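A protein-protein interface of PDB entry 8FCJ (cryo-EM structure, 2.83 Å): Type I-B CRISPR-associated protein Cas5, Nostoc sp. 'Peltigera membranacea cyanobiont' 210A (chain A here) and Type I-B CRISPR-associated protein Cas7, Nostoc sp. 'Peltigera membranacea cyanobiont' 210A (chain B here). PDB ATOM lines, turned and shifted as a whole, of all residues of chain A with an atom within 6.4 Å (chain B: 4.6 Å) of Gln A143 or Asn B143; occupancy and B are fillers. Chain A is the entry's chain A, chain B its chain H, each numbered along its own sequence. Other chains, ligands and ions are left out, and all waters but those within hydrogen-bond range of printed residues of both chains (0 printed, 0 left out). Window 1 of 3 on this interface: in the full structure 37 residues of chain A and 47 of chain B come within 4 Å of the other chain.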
ATOM      1  N   VAL A  11      -1.181  17.657 -10.983  1.00  0.00           N
ATOM      2  CA  VAL A  11      -0.045  18.264 -10.230  1.00  0.00           C
ATOM      3  C   VAL A  11       1.268  17.853 -10.906  1.00  0.00           C
ATOM      4  O   VAL A  11       1.493  16.639 -11.078  1.00  0.00           O
ATOM      5  CB  VAL A  11      -0.065  17.850  -8.746  1.00  0.00           C
ATOM      6  CG1 VAL A  11       0.484  18.947  -7.847  1.00  0.00           C
ATOM      7  CG2 VAL A  11      -1.455  17.433  -8.291  1.00  0.00           C
ATOM      8  N   PRO A  12       2.139  18.812 -11.292  1.00  0.00           N
ATOM      9  CA  PRO A  12       3.414  18.493 -11.938  1.00  0.00           C
ATOM     10  C   PRO A  12       4.295  17.635 -11.020  1.00  0.00           C
ATOM     11  O   PRO A  12       4.875  16.678 -11.501  1.00  0.00           O
ATOM     12  CB  PRO A  12       4.075  19.863 -12.145  1.00  0.00           C
ATOM     13  CG  PRO A  12       2.920  20.840 -12.130  1.00  0.00           C
ATOM     14  CD  PRO A  12       1.937  20.254 -11.139  1.00  0.00           C
ATOM     15  N   PHE A  13       4.373  17.998  -9.737  1.00  0.00           N
ATOM     16  CA  PHE A  13       5.196  17.229  -8.766  1.00  0.00           C
ATOM     17  C   PHE A  13       4.419  17.066  -7.456  1.00  0.00           C
ATOM     18  O   PHE A  13       3.732  18.022  -7.047  1.00  0.00           O
ATOM     19  CB  PHE A  13       6.547  17.916  -8.547  1.00  0.00           C
ATOM     20  CG  PHE A  13       7.467  17.843  -9.737  1.00  0.00           C
ATOM     21  CD1 PHE A  13       8.096  16.655 -10.074  1.00  0.00           C
ATOM     22  CD2 PHE A  13       7.688  18.954 -10.534  1.00  0.00           C
ATOM     23  CE1 PHE A  13       8.936  16.584 -11.173  1.00  0.00           C
ATOM     24  CE2 PHE A  13       8.527  18.882 -11.634  1.00  0.00           C
ATOM     25  CZ  PHE A  13       9.151  17.697 -11.950  1.00  0.00           C
ATOM     26  N   THR A  14       4.526  15.892  -6.827  1.00  0.00           N
ATOM     27  CA  THR A  14       3.777  15.622  -5.572  1.00  0.00           C
ATOM     28  C   THR A  14       4.603  14.708  -4.662  1.00  0.00           C
ATOM     29  O   THR A  14       5.199  13.746  -5.183  1.00  0.00           O
ATOM     30  CB  THR A  14       2.413  14.989  -5.870  1.00  0.00           C
ATOM     31  OG1 THR A  14       2.460  14.407  -7.175  1.00  0.00           O
ATOM     32  CG2 THR A  14       1.274  15.981  -5.794  1.00  0.00           C
ATOM     33  N   THR A  15       4.630  14.998  -3.357  1.00  0.00           N
ATOM     34  CA  THR A  15       5.351  14.120  -2.396  1.00  0.00           C
ATOM     35  C   THR A  15       4.396  13.721  -1.267  1.00  0.00           C
ATOM     36  O   THR A  15       4.137  14.567  -0.388  1.00  0.00           O
ATOM     37  CB  THR A  15       6.615  14.798  -1.850  1.00  0.00           C
ATOM     38  OG1 THR A  15       7.535  14.946  -2.931  1.00  0.00           O
ATOM     39  CG2 THR A  15       7.267  14.016  -0.732  1.00  0.00           C
ATOM     40  N   PHE A  16       3.936  12.472  -1.254  1.00  0.00           N
ATOM     41  CA  PHE A  16       3.092  11.990  -0.163  1.00  0.00           C
ATOM     42  C   PHE A  16       3.934  11.165   0.795  1.00  0.00           C
ATOM     43  O   PHE A  16       3.817   9.942   0.831  1.00  0.00           O
ATOM     44  CB  PHE A  16       1.936  11.148  -0.695  1.00  0.00           C
ATOM     45  CG  PHE A  16       1.349  11.665  -1.972  1.00  0.00           C
ATOM     46  CD1 PHE A  16       0.774  12.923  -2.023  1.00  0.00           C
ATOM     47  CD2 PHE A  16       1.377  10.898  -3.121  1.00  0.00           C
ATOM     48  CE1 PHE A  16       0.234  13.406  -3.198  1.00  0.00           C
ATOM     49  CE2 PHE A  16       0.840  11.375  -4.299  1.00  0.00           C
ATOM     50  CZ  PHE A  16       0.268  12.630  -4.338  1.00  0.00           C
ATOM     51  N   GLN A  93      14.420  12.822  -0.858  1.00  0.00           N
ATOM     52  CA  GLN A  93      12.971  12.956  -0.851  1.00  0.00           C
ATOM     53  C   GLN A  93      12.438  12.413  -2.167  1.00  0.00           C
ATOM     54  O   GLN A  93      12.909  12.807  -3.237  1.00  0.00           O
ATOM     55  CB  GLN A  93      12.554  14.416  -0.662  1.00  0.00           C
ATOM     56  CG  GLN A  93      11.124  14.594  -0.203  1.00  0.00           C
ATOM     57  CD  GLN A  93      10.543  15.926  -0.622  1.00  0.00           C
ATOM     58  OE1 GLN A  93      10.666  16.334  -1.775  1.00  0.00           O
ATOM     59  NE2 GLN A  93       9.908  16.616   0.316  1.00  0.00           N
ATOM     60  N   GLU A  94      11.465  11.512  -2.089  1.00  0.00           N
ATOM     61  CA  GLU A  94      10.911  10.873  -3.274  1.00  0.00           C
ATOM     62  C   GLU A  94       9.717  11.669  -3.780  1.00  0.00           C
ATOM     63  O   GLU A  94       8.813  11.996  -3.009  1.00  0.00           O
ATOM     64  CB  GLU A  94      10.495   9.436  -2.970  1.00  0.00           C
ATOM     65  CG  GLU A  94      11.641   8.520  -2.610  1.00  0.00           C
ATOM     66  CD  GLU A  94      11.213   7.072  -2.509  1.00  0.00           C
ATOM     67  OE1 GLU A  94       9.994   6.817  -2.456  1.00  0.00           O
ATOM     68  OE2 GLU A  94      12.096   6.190  -2.482  1.00  0.00           O
ATOM     69  N   ILE A  95       9.710  11.967  -5.077  1.00  0.00           N
ATOM     70  CA  ILE A  95       8.653  12.764  -5.682  1.00  0.00           C
ATOM     71  C   ILE A  95       7.985  11.957  -6.786  1.00  0.00           C
ATOM     72  O   ILE A  95       8.545  10.997  -7.320  1.00  0.00           O
ATOM     73  CB  ILE A  95       9.177  14.103  -6.237  1.00  0.00           C
ATOM     74  CG1 ILE A  95      10.034  13.865  -7.478  1.00  0.00           C
ATOM     75  CG2 ILE A  95       9.963  14.848  -5.175  1.00  0.00           C
ATOM     76  CD1 ILE A  95      10.794  15.082  -7.936  1.00  0.00           C
ATOM     77  N   LEU A  96       6.762  12.359  -7.118  1.00  0.00           N
ATOM     78  CA  LEU A  96       5.996  11.775  -8.209  1.00  0.00           C
ATOM     79  C   LEU A  96       5.795  12.832  -9.283  1.00  0.00           C
ATOM     80  O   LEU A  96       5.456  13.978  -8.971  1.00  0.00           O
ATOM     81  CB  LEU A  96       4.644  11.259  -7.717  1.00  0.00           C
ATOM     82  CG  LEU A  96       4.666  10.148  -6.671  1.00  0.00           C
ATOM     83  CD1 LEU A  96       3.253   9.804  -6.251  1.00  0.00           C
ATOM     84  CD2 LEU A  96       5.374   8.925  -7.214  1.00  0.00           C
ATOM     85  N   LEU A 136      -2.736  27.113  -3.500  1.00  0.00           N
ATOM     86  CA  LEU A 136      -3.201  25.736  -3.415  1.00  0.00           C
ATOM     87  C   LEU A 136      -2.087  24.777  -3.810  1.00  0.00           C
ATOM     88  O   LEU A 136      -1.443  24.950  -4.849  1.00  0.00           O
ATOM     89  CB  LEU A 136      -4.418  25.539  -4.317  1.00  0.00           C
ATOM     90  CG  LEU A 136      -5.414  24.457  -3.909  1.00  0.00           C
ATOM     91  CD1 LEU A 136      -5.653  24.489  -2.414  1.00  0.00           C
ATOM     92  CD2 LEU A 136      -6.716  24.641  -4.659  1.00  0.00           C
ATOM     93  N   PHE A 137      -1.863  23.760  -2.982  1.00  0.00           N
ATOM     94  CA  PHE A 137      -0.819  22.782  -3.245  1.00  0.00           C
ATOM     95  C   PHE A 137      -1.272  21.418  -2.750  1.00  0.00           C
ATOM     96  O   PHE A 137      -2.167  21.305  -1.910  1.00  0.00           O
ATOM     97  CB  PHE A 137       0.508  23.175  -2.587  1.00  0.00           C
ATOM     98  CG  PHE A 137       0.451  23.252  -1.085  1.00  0.00           C
ATOM     99  CD1 PHE A 137       0.091  24.426  -0.454  1.00  0.00           C
ATOM    100  CD2 PHE A 137       0.776  22.157  -0.308  1.00  0.00           C
ATOM    101  CE1 PHE A 137       0.047  24.503   0.923  1.00  0.00           C
ATOM    102  CE2 PHE A 137       0.734  22.230   1.068  1.00  0.00           C
ATOM    103  CZ  PHE A 137       0.369  23.403   1.683  1.00  0.00           C
ATOM    104  N   LEU A 138      -0.639  20.379  -3.288  1.00  0.00           N
ATOM    105  CA  LEU A 138      -0.884  18.999  -2.884  1.00  0.00           C
ATOM    106  C   LEU A 138       0.438  18.405  -2.421  1.00  0.00           C
ATOM    107  O   LEU A 138       1.352  18.209  -3.230  1.00  0.00           O
ATOM    108  CB  LEU A 138      -1.481  18.187  -4.030  1.00  0.00           C
ATOM    109  CG  LEU A 138      -2.036  16.815  -3.658  1.00  0.00           C
ATOM    110  CD1 LEU A 138      -3.241  16.964  -2.752  1.00  0.00           C
ATOM    111  CD2 LEU A 138      -2.396  16.029  -4.903  1.00  0.00           C
ATOM    112  N   GLY A 139       0.540  18.118  -1.129  1.00  0.00           N
ATOM    113  CA  GLY A 139       1.783  17.636  -0.563  1.00  0.00           C
ATOM    114  C   GLY A 139       2.556  18.733   0.137  1.00  0.00           C
ATOM    115  O   GLY A 139       2.113  19.251   1.165  1.00  0.00           O
ATOM    116  N   GLU A 140       3.709  19.097  -0.409  1.00  0.00           N
ATOM    117  CA  GLU A 140       4.530  20.154   0.159  1.00  0.00           C
ATOM    118  C   GLU A 140       4.101  21.515  -0.381  1.00  0.00           C
ATOM    119  O   GLU A 140       3.537  21.627  -1.470  1.00  0.00           O
ATOM    120  CB  GLU A 140       6.005  19.909  -0.141  1.00  0.00           C
ATOM    121  CG  GLU A 140       6.740  19.168   0.957  1.00  0.00           C
ATOM    122  CD  GLU A 140       8.085  19.787   1.269  1.00  0.00           C
ATOM    123  OE1 GLU A 140       8.578  20.584   0.443  1.00  0.00           O
ATOM    124  OE2 GLU A 140       8.650  19.478   2.338  1.00  0.00           O
ATOM    125  N   SER A 141       4.396  22.558   0.399  1.00  0.00           N
ATOM    126  CA  SER A 141       3.931  23.901   0.059  1.00  0.00           C
ATOM    127  C   SER A 141       4.477  24.376  -1.279  1.00  0.00           C
ATOM    128  O   SER A 141       3.849  25.206  -1.944  1.00  0.00           O
ATOM    129  CB  SER A 141       4.320  24.887   1.160  1.00  0.00           C
ATOM    130  OG  SER A 141       5.673  24.710   1.545  1.00  0.00           O
ATOM    131  N   ASP A 142       5.638  23.874  -1.689  1.00  0.00           N
ATOM    132  CA  ASP A 142       6.224  24.282  -2.957  1.00  0.00           C
ATOM    133  C   ASP A 142       5.687  23.492  -4.141  1.00  0.00           C
ATOM    134  O   ASP A 142       6.010  23.831  -5.283  1.00  0.00           O
ATOM    135  CB  ASP A 142       7.745  24.148  -2.900  1.00  0.00           C
ATOM    136  CG  ASP A 142       8.369  25.059  -1.868  1.00  0.00           C
ATOM    137  OD1 ASP A 142       7.996  26.250  -1.822  1.00  0.00           O
ATOM    138  OD2 ASP A 142       9.232  24.588  -1.099  1.00  0.00           O
ATOM    139  N   GLN A 143       4.879  22.461  -3.904  1.00  0.00           N
ATOM    140  CA  GLN A 143       4.349  21.622  -4.976  1.00  0.00           C
ATOM    141  C   GLN A 143       2.945  22.107  -5.323  1.00  0.00           C
ATOM    142  O   GLN A 143       1.935  21.534  -4.920  1.00  0.00           O
ATOM    143  CB  GLN A 143       4.367  20.159  -4.563  1.00  0.00           C
ATOM    144  CG  GLN A 143       5.767  19.610  -4.423  1.00  0.00           C
ATOM    145  CD  GLN A 143       5.806  18.300  -3.682  1.00  0.00           C
ATOM    146  OE1 GLN A 143       4.894  17.971  -2.929  1.00  0.00           O
ATOM    147  NE2 GLN A 143       6.871  17.541  -3.890  1.00  0.00           N
ATOM    148  N   LEU A 144       2.899  23.183  -6.101  1.00  0.00           N
ATOM    149  CA  LEU A 144       1.639  23.814  -6.454  1.00  0.00           C
ATOM    150  C   LEU A 144       0.827  22.929  -7.392  1.00  0.00           C
ATOM    151  O   LEU A 144       1.356  22.071  -8.102  1.00  0.00           O
ATOM    152  CB  LEU A 144       1.889  25.169  -7.110  1.00  0.00           C
ATOM    153  CG  LEU A 144       2.735  26.166  -6.322  1.00  0.00           C
ATOM    154  CD1 LEU A 144       2.664  27.525  -6.978  1.00  0.00           C
ATOM    155  CD2 LEU A 144       2.265  26.244  -4.885  1.00  0.00           C
ATOM    156  N   ILE A 145      -0.481  23.157  -7.391  1.00  0.00           N
ATOM    157  CA  ILE A 145      -1.409  22.423  -8.241  1.00  0.00           C
ATOM    158  C   ILE A 145      -1.492  23.123  -9.587  1.00  0.00           C
ATOM    159  O   ILE A 145      -1.714  24.338  -9.654  1.00  0.00           O
ATOM    160  CB  ILE A 145      -2.796  22.331  -7.584  1.00  0.00           C
ATOM    161  CG1 ILE A 145      -2.770  21.347  -6.417  1.00  0.00           C
ATOM    162  CG2 ILE A 145      -3.840  21.917  -8.602  1.00  0.00           C
ATOM    163  CD1 ILE A 145      -4.125  21.101  -5.807  1.00  0.00           C
ATOM    164  N   SER B  57      13.249  23.338  -5.469  1.00  0.00           N
ATOM    165  CA  SER B  57      12.532  24.570  -5.160  1.00  0.00           C
ATOM    166  C   SER B  57      13.251  25.370  -4.084  1.00  0.00           C
ATOM    167  O   SER B  57      13.254  26.607  -4.113  1.00  0.00           O
ATOM    168  CB  SER B  57      11.105  24.246  -4.724  1.00  0.00           C
ATOM    169  OG  SER B  57      11.095  23.209  -3.762  1.00  0.00           O
ATOM    170  N   ILE B  60      15.781  27.832  -5.610  1.00  0.00           N
ATOM    171  CA  ILE B  60      15.257  29.088  -6.136  1.00  0.00           C
ATOM    172  C   ILE B  60      14.776  29.985  -5.002  1.00  0.00           C
ATOM    173  O   ILE B  60      14.920  31.213  -5.060  1.00  0.00           O
ATOM    174  CB  ILE B  60      14.148  28.812  -7.163  1.00  0.00           C
ATOM    175  CG1 ILE B  60      14.563  27.666  -8.083  1.00  0.00           C
ATOM    176  CG2 ILE B  60      13.874  30.053  -7.984  1.00  0.00           C
ATOM    177  CD1 ILE B  60      13.413  27.003  -8.788  1.00  0.00           C
ATOM    178  N   GLY B 141       5.141  30.300  -3.155  1.00  0.00           N
ATOM    179  CA  GLY B 141       5.514  28.917  -3.359  1.00  0.00           C
ATOM    180  C   GLY B 141       5.929  28.679  -4.794  1.00  0.00           C
ATOM    181  O   GLY B 141       5.193  29.035  -5.717  1.00  0.00           O
ATOM    182  N   MET B 142       7.106  28.099  -5.005  1.00  0.00           N
ATOM    183  CA  MET B 142       7.606  27.841  -6.348  1.00  0.00           C
ATOM    184  C   MET B 142       7.898  26.362  -6.518  1.00  0.00           C
ATOM    185  O   MET B 142       8.531  25.748  -5.655  1.00  0.00           O
ATOM    186  CB  MET B 142       8.867  28.654  -6.644  1.00  0.00           C
ATOM    187  CG  MET B 142       9.631  29.088  -5.420  1.00  0.00           C
ATOM    188  SD  MET B 142      10.979  30.178  -5.888  1.00  0.00           S
ATOM    189  CE  MET B 142      10.088  31.403  -6.838  1.00  0.00           C
ATOM    190  N   ASN B 143       7.434  25.798  -7.627  1.00  0.00           N
ATOM    191  CA  ASN B 143       7.773  24.430  -7.969  1.00  0.00           C
ATOM    192  C   ASN B 143       9.219  24.350  -8.440  1.00  0.00           C
ATOM    193  O   ASN B 143       9.847  25.355  -8.782  1.00  0.00           O
ATOM    194  CB  ASN B 143       6.830  23.901  -9.046  1.00  0.00           C
ATOM    195  CG  ASN B 143       6.072  22.674  -8.600  1.00  0.00           C
ATOM    196  OD1 ASN B 143       6.316  22.142  -7.520  1.00  0.00           O
ATOM    197  ND2 ASN B 143       5.140  22.221  -9.426  1.00  0.00           N
ATOM    198  N   MET B 144       9.752  23.134  -8.450  1.00  0.00           N
ATOM    199  CA  MET B 144      11.135  22.944  -8.856  1.00  0.00           C
ATOM    200  C   MET B 144      11.296  23.181 -10.351  1.00  0.00           C
ATOM    201  O   MET B 144      10.379  22.957 -11.144  1.00  0.00           O
ATOM    202  CB  MET B 144      11.614  21.542  -8.489  1.00  0.00           C
ATOM    203  CG  MET B 144      10.966  20.426  -9.273  1.00  0.00           C
ATOM    204  SD  MET B 144      11.314  18.815  -8.552  1.00  0.00           S
ATOM    205  CE  MET B 144      11.667  19.277  -6.861  1.00  0.00           C
ATOM    206  N   ALA B 145      12.477  23.658 -10.730  1.00  0.00           N
ATOM    207  CA  ALA B 145      12.784  23.906 -12.129  1.00  0.00           C
ATOM    208  C   ALA B 145      13.242  22.624 -12.806  1.00  0.00           C
ATOM    209  O   ALA B 145      14.057  21.875 -12.261  1.00  0.00           O
ATOM    210  CB  ALA B 145      13.863  24.979 -12.259  1.00  0.00           C
ATOM    211  N   TYR B 182      10.478  26.939 -14.584  1.00  0.00           N
ATOM    212  CA  TYR B 182       9.903  26.683 -13.275  1.00  0.00           C
ATOM    213  C   TYR B 182       8.615  27.475 -13.128  1.00  0.00           C
ATOM    214  O   TYR B 182       8.354  28.426 -13.868  1.00  0.00           O
ATOM    215  CB  TYR B 182      10.877  27.026 -12.141  1.00  0.00           C
ATOM    216  CG  TYR B 182      11.278  28.479 -12.061  1.00  0.00           C
ATOM    217  CD1 TYR B 182      12.339  28.967 -12.807  1.00  0.00           C
ATOM    218  CD2 TYR B 182      10.609  29.358 -11.224  1.00  0.00           C
ATOM    219  CE1 TYR B 182      12.714  30.287 -12.729  1.00  0.00           C
ATOM    220  CE2 TYR B 182      10.976  30.683 -11.143  1.00  0.00           C
ATOM    221  CZ  TYR B 182      12.030  31.142 -11.897  1.00  0.00           C
ATOM    222  OH  TYR B 182      12.402  32.462 -11.820  1.00  0.00           O
ATOM    223  N   TYR B 183       7.808  27.061 -12.160  1.00  0.00           N
ATOM    224  CA  TYR B 183       6.495  27.636 -11.922  1.00  0.00           C
ATOM    225  C   TYR B 183       6.408  28.117 -10.484  1.00  0.00           C
ATOM    226  O   TYR B 183       6.772  27.392  -9.554  1.00  0.00           O
ATOM    227  CB  TYR B 183       5.401  26.611 -12.209  1.00  0.00           C
ATOM    228  CG  TYR B 183       4.004  27.064 -11.869  1.00  0.00           C
ATOM    229  CD1 TYR B 183       3.425  28.139 -12.523  1.00  0.00           C
ATOM    230  CD2 TYR B 183       3.256  26.403 -10.908  1.00  0.00           C
ATOM    231  CE1 TYR B 183       2.145  28.548 -12.222  1.00  0.00           C
ATOM    232  CE2 TYR B 183       1.978  26.806 -10.600  1.00  0.00           C
ATOM    233  CZ  TYR B 183       1.427  27.878 -11.260  1.00  0.00           C
ATOM    234  OH  TYR B 183       0.151  28.281 -10.955  1.00  0.00           O
ATOM    235  N   TYR B 240       3.300  24.723 -16.574  1.00  0.00           N
ATOM    236  CA  TYR B 240       4.445  24.434 -17.439  1.00  0.00           C
ATOM    237  C   TYR B 240       3.965  24.512 -18.883  1.00  0.00           C
ATOM    238  O   TYR B 240       3.609  23.499 -19.489  1.00  0.00           O
ATOM    239  CB  TYR B 240       5.050  23.082 -17.101  1.00  0.00           C
ATOM    240  CG  TYR B 240       5.773  23.072 -15.774  1.00  0.00           C
ATOM    241  CD1 TYR B 240       5.095  22.809 -14.594  1.00  0.00           C
ATOM    242  CD2 TYR B 240       7.130  23.338 -15.700  1.00  0.00           C
ATOM    243  CE1 TYR B 240       5.751  22.805 -13.381  1.00  0.00           C
ATOM    244  CE2 TYR B 240       7.792  23.335 -14.493  1.00  0.00           C
ATOM    245  CZ  TYR B 240       7.099  23.070 -13.338  1.00  0.00           C
ATOM    246  OH  TYR B 240       7.759  23.067 -12.134  1.00  0.00           O
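OD1 of Asn B143 sits close to O of Asp A142, 2.8 Å away. The backbone carbonyl oxygen (O) of Asp A142 lies close to the backbone carbonyl oxygen (O) of Met B142 (3.2 Å).
Asn B143 touches Pro A12 (ND2 to CB, 3.8 Å). CB of Pro A12 touches CE1 of Tyr B240, at 3.6 Å. Phe A13 touches Met B144 (CE2 to CG, 3.7 Å). Met B144 touches Ile A95. OG of Ser B57 touches OD2 of Asp A142, at 3.5 Å. Asp A142 touches Gly B141. Gln A143 touches Asn B143 (CA to OD1, 3.3 Å). Leu A144 touches Gly B141. Leu A144 touches Asn B143. Tyr B183 touches Leu A144 (CE2 to CD1, 3.8 Å).
The side-chain hydroxyl (OG1) of Thr A15 is in hydrogen-bond range of the side-chain amide nitrogen (NE2) of Gln A143 (2.8 Å). The backbone NH of Leu A138 sits at hydrogen-bond distance from the backbone carbonyl oxygen of Gln A143, 3.3 Å away. The backbone NH of Glu A140 is in hydrogen-bond range of the side-chain amide oxygen of Gln A143 (3.0 Å). The backbone NH (N) of Asn B143 sits at hydrogen-bond distance from the backbone carbonyl oxygen (O) of Tyr B183 (2.6 Å). O of Met B144 lies within hydrogen-bond range of OH of Tyr B240 (2.8 Å).
Printed residues of chain B that touch a printed residue of chain A: Ser B57, Gly B141, Met B142, Asn B143, Met B144, Tyr B183 and Tyr B240. Hydrophobic or aromatic side chains of chain B that line the printed part of chain A: Met B144, Tyr B183 and Tyr B240. Along chain B the printed residues that touch a printed residue of chain A span positions 57 to 240. Of the 20 printed residues of chain A, 6 touch a printed residue of chain B. Among the printed residues, 12 pairs touch across the chains.
Gln A143 touches one residue of chain B. Of chain A, only Pro A12, Asp A142, Gln A143 and Leu A144 come within 4 Å of Asn B143. Of the printed residues of chain A, Met B142 touches Asp A142 (3.2 Å). Printed residues of chain B within 4 Å of Asp A142: Ser B57 (3.5 Å), Gly B141 (3.95 Å), Met B142 (3.2 Å) and Asn B143 (2.8 Å). Of the printed residues of chain A, Gly B141 touches Asp A142 (3.95 Å) and Leu A144 (3.2 Å). Printed residues of chain B within 4 Å of Pro A12: Asn B143 and Tyr B240. Printed residues of chain A within 4 Å of Met B144: Phe A13 and Ile A95. Tyr B182 touches none of the printed residues of chain A. The nearest residue of chain A that does not touch Asn B143 is Phe A13 (4.3 Å).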
